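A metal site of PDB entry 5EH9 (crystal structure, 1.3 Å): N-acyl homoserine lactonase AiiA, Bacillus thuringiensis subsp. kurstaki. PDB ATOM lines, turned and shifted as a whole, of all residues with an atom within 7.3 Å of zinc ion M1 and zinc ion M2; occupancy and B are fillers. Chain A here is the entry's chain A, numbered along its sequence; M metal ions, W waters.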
ATOM      1  N   LEU A  19      -8.354  -2.968   9.067  1.00  0.00           N
ATOM      2  CA  LEU A  19      -9.538  -2.288   8.577  1.00  0.00           C
ATOM      3  C   LEU A  19      -9.273  -1.825   7.145  1.00  0.00           C
ATOM      4  O   LEU A  19      -8.157  -1.528   6.772  1.00  0.00           O
ATOM      5  CB  LEU A  19      -9.810  -1.066   9.448  1.00  0.00           C
ATOM      6  CG  LEU A  19     -10.261  -1.153  10.891  1.00  0.00           C
ATOM      7  CD1 LEU A  19     -10.649   0.284  11.356  1.00  0.00           C
ATOM      8  CD2 LEU A  19     -11.397  -2.147  11.178  1.00  0.00           C
ATOM      9  N   PRO A  37      -2.922  -0.273  14.833  1.00  0.00           N
ATOM     10  CA  PRO A  37      -2.652  -0.596  16.215  1.00  0.00           C
ATOM     11  C   PRO A  37      -3.920  -0.627  17.058  1.00  0.00           C
ATOM     12  O   PRO A  37      -4.825   0.220  16.825  1.00  0.00           O
ATOM     13  CB  PRO A  37      -1.749   0.479  16.672  1.00  0.00           C
ATOM     14  CG  PRO A  37      -2.128   1.678  15.838  1.00  0.00           C
ATOM     15  CD  PRO A  37      -2.472   1.093  14.484  1.00  0.00           C
ATOM     16  N   VAL A  38      -4.013  -1.516  18.029  1.00  0.00           N
ATOM     17  CA  VAL A  38      -4.972  -1.483  19.089  1.00  0.00           C
ATOM     18  C   VAL A  38      -4.197  -1.168  20.346  1.00  0.00           C
ATOM     19  O   VAL A  38      -3.160  -1.765  20.635  1.00  0.00           O
ATOM     20  CB  VAL A  38      -5.744  -2.822  19.187  1.00  0.00           C
ATOM     21  CG1 VAL A  38      -6.630  -2.831  20.425  1.00  0.00           C
ATOM     22  CG2 VAL A  38      -6.563  -3.063  17.932  1.00  0.00           C
ATOM     23  N   TRP A  39      -4.725  -0.202  21.105  1.00  0.00           N
ATOM     24  CA  TRP A  39      -4.048   0.273  22.316  1.00  0.00           C
ATOM     25  C   TRP A  39      -4.855   0.123  23.573  1.00  0.00           C
ATOM     26  O   TRP A  39      -6.055   0.237  23.562  1.00  0.00           O
ATOM     27  CB  TRP A  39      -3.843   1.827  22.208  1.00  0.00           C
ATOM     28  CG  TRP A  39      -2.994   2.290  21.078  1.00  0.00           C
ATOM     29  CD1 TRP A  39      -3.433   2.973  19.950  1.00  0.00           C
ATOM     30  CD2 TRP A  39      -1.576   2.248  20.998  1.00  0.00           C
ATOM     31  NE1 TRP A  39      -2.360   3.294  19.157  1.00  0.00           N
ATOM     32  CE2 TRP A  39      -1.206   2.893  19.798  1.00  0.00           C
ATOM     33  CE3 TRP A  39      -0.563   1.790  21.828  1.00  0.00           C
ATOM     34  CZ2 TRP A  39       0.102   3.066  19.453  1.00  0.00           C
ATOM     35  CZ3 TRP A  39       0.756   1.936  21.459  1.00  0.00           C
ATOM     36  CH2 TRP A  39       1.077   2.541  20.288  1.00  0.00           C
ATOM     37  N   ASP A  53      -9.160   1.176  28.466  1.00  0.00           N
ATOM     38  CA  ASP A  53      -9.529   0.176  27.467  1.00  0.00           C
ATOM     39  C   ASP A  53      -8.841  -1.176  27.732  1.00  0.00           C
ATOM     40  O   ASP A  53      -7.906  -1.306  28.499  1.00  0.00           O
ATOM     41  CB  ASP A  53      -9.273   0.717  26.061  1.00  0.00           C
ATOM     42  CG  ASP A  53     -10.337   1.812  25.707  1.00  0.00           C
ATOM     43  OD1 ASP A  53     -11.337   1.925  26.411  1.00  0.00           O
ATOM     44  OD2 ASP A  53     -10.058   2.540  24.702  1.00  0.00           O
ATOM     45  N   SER A 106     -13.251   3.954  26.837  1.00  0.00           N
ATOM     46  CA  SER A 106     -13.436   5.079  25.921  1.00  0.00           C
ATOM     47  C   SER A 106     -14.779   4.886  25.211  1.00  0.00           C
ATOM     48  O   SER A 106     -15.539   5.849  24.975  1.00  0.00           O
ATOM     49  CB  SER A 106     -12.304   5.139  24.933  1.00  0.00           C
ATOM     50  OG  SER A 106     -12.254   3.991  24.099  1.00  0.00           O
ATOM     51  N   HIS A 107     -15.044   3.636  24.793  1.00  0.00           N
ATOM     52  CA  HIS A 107     -16.266   3.264  24.174  1.00  0.00           C
ATOM     53  C   HIS A 107     -16.295   1.696  24.165  1.00  0.00           C
ATOM     54  O   HIS A 107     -15.339   1.113  24.634  1.00  0.00           O
ATOM     55  CB  HIS A 107     -16.440   3.847  22.774  1.00  0.00           C
ATOM     56  CG  HIS A 107     -15.412   3.528  21.760  1.00  0.00           C
ATOM     57  ND1 HIS A 107     -14.062   3.679  21.936  1.00  0.00           N
ATOM     58  CD2 HIS A 107     -15.565   3.133  20.447  1.00  0.00           C
ATOM     59  CE1 HIS A 107     -13.434   3.447  20.800  1.00  0.00           C
ATOM     60  NE2 HIS A 107     -14.333   3.087  19.883  1.00  0.00           N
ATOM     61  N   LEU A 108     -17.385   1.151  23.696  1.00  0.00           N
ATOM     62  CA  LEU A 108     -17.600  -0.292  23.801  1.00  0.00           C
ATOM     63  C   LEU A 108     -17.457  -1.048  22.516  1.00  0.00           C
ATOM     64  O   LEU A 108     -17.883  -2.215  22.419  1.00  0.00           O
ATOM     65  CB  LEU A 108     -18.921  -0.609  24.541  1.00  0.00           C
ATOM     66  CG  LEU A 108     -19.056  -0.068  25.999  1.00  0.00           C
ATOM     67  CD1 LEU A 108     -20.460  -0.298  26.493  1.00  0.00           C
ATOM     68  CD2 LEU A 108     -17.953  -0.649  26.908  1.00  0.00           C
ATOM     69  N   HIS A 109     -16.804  -0.485  21.531  1.00  0.00           N
ATOM     70  CA  HIS A 109     -16.339  -1.239  20.366  1.00  0.00           C
ATOM     71  C   HIS A 109     -15.479  -2.382  20.800  1.00  0.00           C
ATOM     72  O   HIS A 109     -14.778  -2.353  21.784  1.00  0.00           O
ATOM     73  CB  HIS A 109     -15.632  -0.351  19.364  1.00  0.00           C
ATOM     74  CG  HIS A 109     -16.583   0.566  18.633  1.00  0.00           C
ATOM     75  ND1 HIS A 109     -16.126   1.604  17.810  1.00  0.00           N
ATOM     76  CD2 HIS A 109     -17.924   0.601  18.565  1.00  0.00           C
ATOM     77  CE1 HIS A 109     -17.180   2.225  17.291  1.00  0.00           C
ATOM     78  NE2 HIS A 109     -18.265   1.672  17.760  1.00  0.00           N
ATOM     79  N   PHE A 110     -15.448  -3.422  19.964  1.00  0.00           N
ATOM     80  CA  PHE A 110     -14.766  -4.700  20.315  1.00  0.00           C
ATOM     81  C   PHE A 110     -13.312  -4.569  20.582  1.00  0.00           C
ATOM     82  O   PHE A 110     -12.728  -5.384  21.329  1.00  0.00           O
ATOM     83  CB  PHE A 110     -15.087  -5.804  19.312  1.00  0.00           C
ATOM     84  CG  PHE A 110     -14.127  -5.852  18.190  1.00  0.00           C
ATOM     85  CD1 PHE A 110     -14.083  -4.869  17.212  1.00  0.00           C
ATOM     86  CD2 PHE A 110     -13.211  -6.821  18.160  1.00  0.00           C
ATOM     87  CE1 PHE A 110     -13.110  -4.896  16.231  1.00  0.00           C
ATOM     88  CE2 PHE A 110     -12.312  -6.933  17.089  1.00  0.00           C
ATOM     89  CZ  PHE A 110     -12.221  -5.927  16.164  1.00  0.00           C
ATOM     90  N   ASP A 111     -12.665  -3.573  19.903  1.00  0.00           N
ATOM     91  CA  ASP A 111     -11.279  -3.315  20.096  1.00  0.00           C
ATOM     92  C   ASP A 111     -10.881  -2.456  21.278  1.00  0.00           C
ATOM     93  O   ASP A 111      -9.714  -2.237  21.524  1.00  0.00           O
ATOM     94  CB  ASP A 111     -10.633  -2.770  18.786  1.00  0.00           C
ATOM     95  CG  ASP A 111     -11.287  -1.448  18.299  1.00  0.00           C
ATOM     96  OD1 ASP A 111     -12.554  -1.444  18.266  1.00  0.00           O
ATOM     97  OD2 ASP A 111     -10.539  -0.509  17.934  1.00  0.00           O
ATOM     98  N   HIS A 112     -11.895  -2.107  22.066  1.00  0.00           N
ATOM     99  CA  HIS A 112     -11.723  -1.314  23.249  1.00  0.00           C
ATOM    100  C   HIS A 112     -12.311  -1.877  24.516  1.00  0.00           C
ATOM    101  O   HIS A 112     -11.842  -1.528  25.611  1.00  0.00           O
ATOM    102  CB  HIS A 112     -12.365   0.103  23.018  1.00  0.00           C
ATOM    103  CG  HIS A 112     -11.720   0.816  21.909  1.00  0.00           C
ATOM    104  ND1 HIS A 112     -10.718   1.734  22.095  1.00  0.00           N
ATOM    105  CD2 HIS A 112     -11.892   0.703  20.592  1.00  0.00           C
ATOM    106  CE1 HIS A 112     -10.253   2.107  20.926  1.00  0.00           C
ATOM    107  NE2 HIS A 112     -10.993   1.521  19.988  1.00  0.00           N
ATOM    108  N   GLU A 130     -23.138   5.487  25.689  1.00  0.00           N
ATOM    109  CA  GLU A 130     -22.432   4.353  25.113  1.00  0.00           C
ATOM    110  C   GLU A 130     -23.020   3.036  25.593  1.00  0.00           C
ATOM    111  O   GLU A 130     -23.269   2.087  24.837  1.00  0.00           O
ATOM    112  CB  GLU A 130     -20.949   4.411  25.462  1.00  0.00           C
ATOM    113  CG  GLU A 130     -20.136   3.368  24.716  1.00  0.00           C
ATOM    114  CD  GLU A 130     -19.990   3.543  23.214  1.00  0.00           C
ATOM    115  OE1 GLU A 130     -20.320   4.663  22.725  1.00  0.00           O
ATOM    116  OE2 GLU A 130     -19.574   2.603  22.540  1.00  0.00           O
ATOM    117  N   HIS A 172     -17.989   9.138  16.805  1.00  0.00           N
ATOM    118  CA  HIS A 172     -17.473   7.853  16.341  1.00  0.00           C
ATOM    119  C   HIS A 172     -18.321   6.696  16.850  1.00  0.00           C
ATOM    120  O   HIS A 172     -18.585   5.701  16.136  1.00  0.00           O
ATOM    121  CB  HIS A 172     -16.025   7.695  16.801  1.00  0.00           C
ATOM    122  CG  HIS A 172     -15.506   6.270  16.597  1.00  0.00           C
ATOM    123  ND1 HIS A 172     -15.158   5.705  15.371  1.00  0.00           N
ATOM    124  CD2 HIS A 172     -15.267   5.307  17.509  1.00  0.00           C
ATOM    125  CE1 HIS A 172     -14.760   4.436  15.544  1.00  0.00           C
ATOM    126  NE2 HIS A 172     -14.780   4.195  16.834  1.00  0.00           N
ATOM    127  N   SER A 173     -18.766   6.795  18.116  1.00  0.00           N
ATOM    128  CA  SER A 173     -19.760   5.960  18.749  1.00  0.00           C
ATOM    129  C   SER A 173     -20.691   6.859  19.554  1.00  0.00           C
ATOM    130  O   SER A 173     -20.304   8.027  19.832  1.00  0.00           O
ATOM    131  CB  SER A 173     -19.120   4.863  19.585  1.00  0.00           C
ATOM    132  OG  SER A 173     -18.556   5.392  20.791  1.00  0.00           O
ATOM    133  N   HIS A 176     -18.826   7.924  22.911  1.00  0.00           N
ATOM    134  CA  HIS A 176     -17.410   7.945  22.936  1.00  0.00           C
ATOM    135  C   HIS A 176     -16.813   9.028  23.852  1.00  0.00           C
ATOM    136  O   HIS A 176     -17.367  10.176  23.888  1.00  0.00           O
ATOM    137  CB  HIS A 176     -16.840   8.183  21.495  1.00  0.00           C
ATOM    138  CG  HIS A 176     -15.378   8.089  21.383  1.00  0.00           C
ATOM    139  ND1 HIS A 176     -14.527   9.139  21.656  1.00  0.00           N
ATOM    140  CD2 HIS A 176     -14.550   7.032  21.133  1.00  0.00           C
ATOM    141  CE1 HIS A 176     -13.274   8.732  21.624  1.00  0.00           C
ATOM    142  NE2 HIS A 176     -13.258   7.439  21.291  1.00  0.00           N
ATOM    143  N   ILE A 193      -8.393   9.001  21.519  1.00  0.00           N
ATOM    144  CA  ILE A 193      -8.945   7.705  21.238  1.00  0.00           C
ATOM    145  C   ILE A 193      -9.581   7.846  19.881  1.00  0.00           C
ATOM    146  O   ILE A 193      -8.931   8.383  18.967  1.00  0.00           O
ATOM    147  CB  ILE A 193      -9.833   7.146  22.350  1.00  0.00           C
ATOM    148  CG1 ILE A 193      -9.327   7.439  23.742  1.00  0.00           C
ATOM    149  CG2 ILE A 193      -9.973   5.614  22.171  1.00  0.00           C
ATOM    150  CD1 ILE A 193      -8.020   6.813  24.169  1.00  0.00           C
ATOM    151  N   ASP A 194     -10.778   7.314  19.678  1.00  0.00           N
ATOM    152  CA  ASP A 194     -11.351   7.230  18.340  1.00  0.00           C
ATOM    153  C   ASP A 194     -12.190   8.425  17.955  1.00  0.00           C
ATOM    154  O   ASP A 194     -12.948   8.408  16.953  1.00  0.00           O
ATOM    155  CB  ASP A 194     -12.092   5.919  18.136  1.00  0.00           C
ATOM    156  CG  ASP A 194     -11.186   4.645  18.096  1.00  0.00           C
ATOM    157  OD1 ASP A 194      -9.952   4.837  18.297  1.00  0.00           O
ATOM    158  OD2 ASP A 194     -11.832   3.529  17.923  1.00  0.00           O
ATOM    159  N   TYR A 197      -9.164   8.788  14.356  1.00  0.00           N
ATOM    160  CA  TYR A 197      -8.248   7.661  14.126  1.00  0.00           C
ATOM    161  C   TYR A 197      -6.840   8.119  13.855  1.00  0.00           C
ATOM    162  O   TYR A 197      -5.852   7.588  14.380  1.00  0.00           O
ATOM    163  CB  TYR A 197      -8.678   6.756  12.949  1.00  0.00           C
ATOM    164  CG  TYR A 197      -9.860   5.872  13.148  1.00  0.00           C
ATOM    165  CD1 TYR A 197     -10.488   5.633  14.345  1.00  0.00           C
ATOM    166  CD2 TYR A 197     -10.331   5.224  12.102  1.00  0.00           C
ATOM    167  CE1 TYR A 197     -11.493   4.693  14.445  1.00  0.00           C
ATOM    168  CE2 TYR A 197     -11.368   4.332  12.190  1.00  0.00           C
ATOM    169  CZ  TYR A 197     -11.906   3.957  13.353  1.00  0.00           C
ATOM    170  OH  TYR A 197     -12.869   3.008  13.393  1.00  0.00           O
ATOM    171  N   ALA A 209     -14.540   6.377   9.949  1.00  0.00           N
ATOM    172  CA  ALA A 209     -15.647   5.531  10.358  1.00  0.00           C
ATOM    173  C   ALA A 209     -16.256   5.999  11.643  1.00  0.00           C
ATOM    174  O   ALA A 209     -15.526   6.308  12.602  1.00  0.00           O
ATOM    175  CB  ALA A 209     -15.164   4.129  10.581  1.00  0.00           C
ATOM    176  N   GLY A 237      -6.118   7.644  17.722  1.00  0.00           N
ATOM    177  CA  GLY A 237      -6.529   6.332  18.106  1.00  0.00           C
ATOM    178  C   GLY A 237      -5.971   5.178  17.334  1.00  0.00           C
ATOM    179  O   GLY A 237      -5.793   4.068  17.905  1.00  0.00           O
ATOM    180  N   HIS A 238      -5.882   5.309  16.036  1.00  0.00           N
ATOM    181  CA  HIS A 238      -5.462   4.159  15.189  1.00  0.00           C
ATOM    182  C   HIS A 238      -4.678   4.687  13.994  1.00  0.00           C
ATOM    183  O   HIS A 238      -5.102   4.654  12.832  1.00  0.00           O
ATOM    184  CB  HIS A 238      -6.737   3.425  14.667  1.00  0.00           C
ATOM    185  CG  HIS A 238      -7.551   2.702  15.687  1.00  0.00           C
ATOM    186  ND1 HIS A 238      -7.138   1.560  16.373  1.00  0.00           N
ATOM    187  CD2 HIS A 238      -8.842   2.869  16.003  1.00  0.00           C
ATOM    188  CE1 HIS A 238      -8.117   1.125  17.122  1.00  0.00           C
ATOM    189  NE2 HIS A 238      -9.162   1.927  16.925  1.00  0.00           N
HETATM  190 ZN    ZN M   1     -10.974   1.696  17.930  1.00  0.00          ZN
HETATM  191 ZN    ZN M   2     -14.201   2.536  17.864  1.00  0.00          ZN
HETATM  192  O   HOH W   1     -12.821   1.238  17.258  1.00  0.00           O
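Of the 22 residues printed, 5 come within 4 Å of zinc ion M2. The nearest printed residue that does not touch zinc ion M2 is Asp 111 (4.3 Å).
The backbone NH (N) of Asp 194 lies within hydrogen-bond range of a ring nitrogen (NE2) of His 176 (3.0 Å). ND1 of His 172 is in hydrogen-bond range of O of Ala 209, at 2.9 Å. A ring nitrogen (ND1) of His 112 lies within hydrogen-bond range of the side-chain carboxylate (OD2) of Asp 53. ND1 of His 112 is in hydrogen-bond range of OG of Ser 106 (3.4 Å). O of Tyr 197 lies within hydrogen-bond range of N of His 238, 2.8 Å away. A ring nitrogen (ND1) of His 238 lies within hydrogen-bond range of the backbone carbonyl oxygen (O) of Pro 37 (2.7 Å). A ring nitrogen (ND1) of His 107 is in hydrogen-bond range of the side-chain hydroxyl (OG) of Ser 106 (2.8 Å).
Zinc ion M1 is bound by water W1 (2.0 Å), OD2 of Asp 194 (2.0 Å), NE2 of His 112 (2.1 Å), NE2 of His 238 (2.1 Å) and OD2 of Asp 111 (2.2 Å). Zinc ion M1 has five donor atoms within binding distance.
Of the 22 residues printed, 4 come within 4 Å of zinc ion M1.
Water W1 binds zinc ion M2, at 2.0 Å. A ring nitrogen (NE2) of His 172 is bound to zinc ion M2. A ring nitrogen (NE2) of His 107 binds zinc ion M2, at 2.1 Å. ND1 of His 109 is bound to zinc ion M2, 2.1 Å away. OD2 of Asp 194 binds zinc ion M2. Zinc ion M2 has five donor atoms within binding distance.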
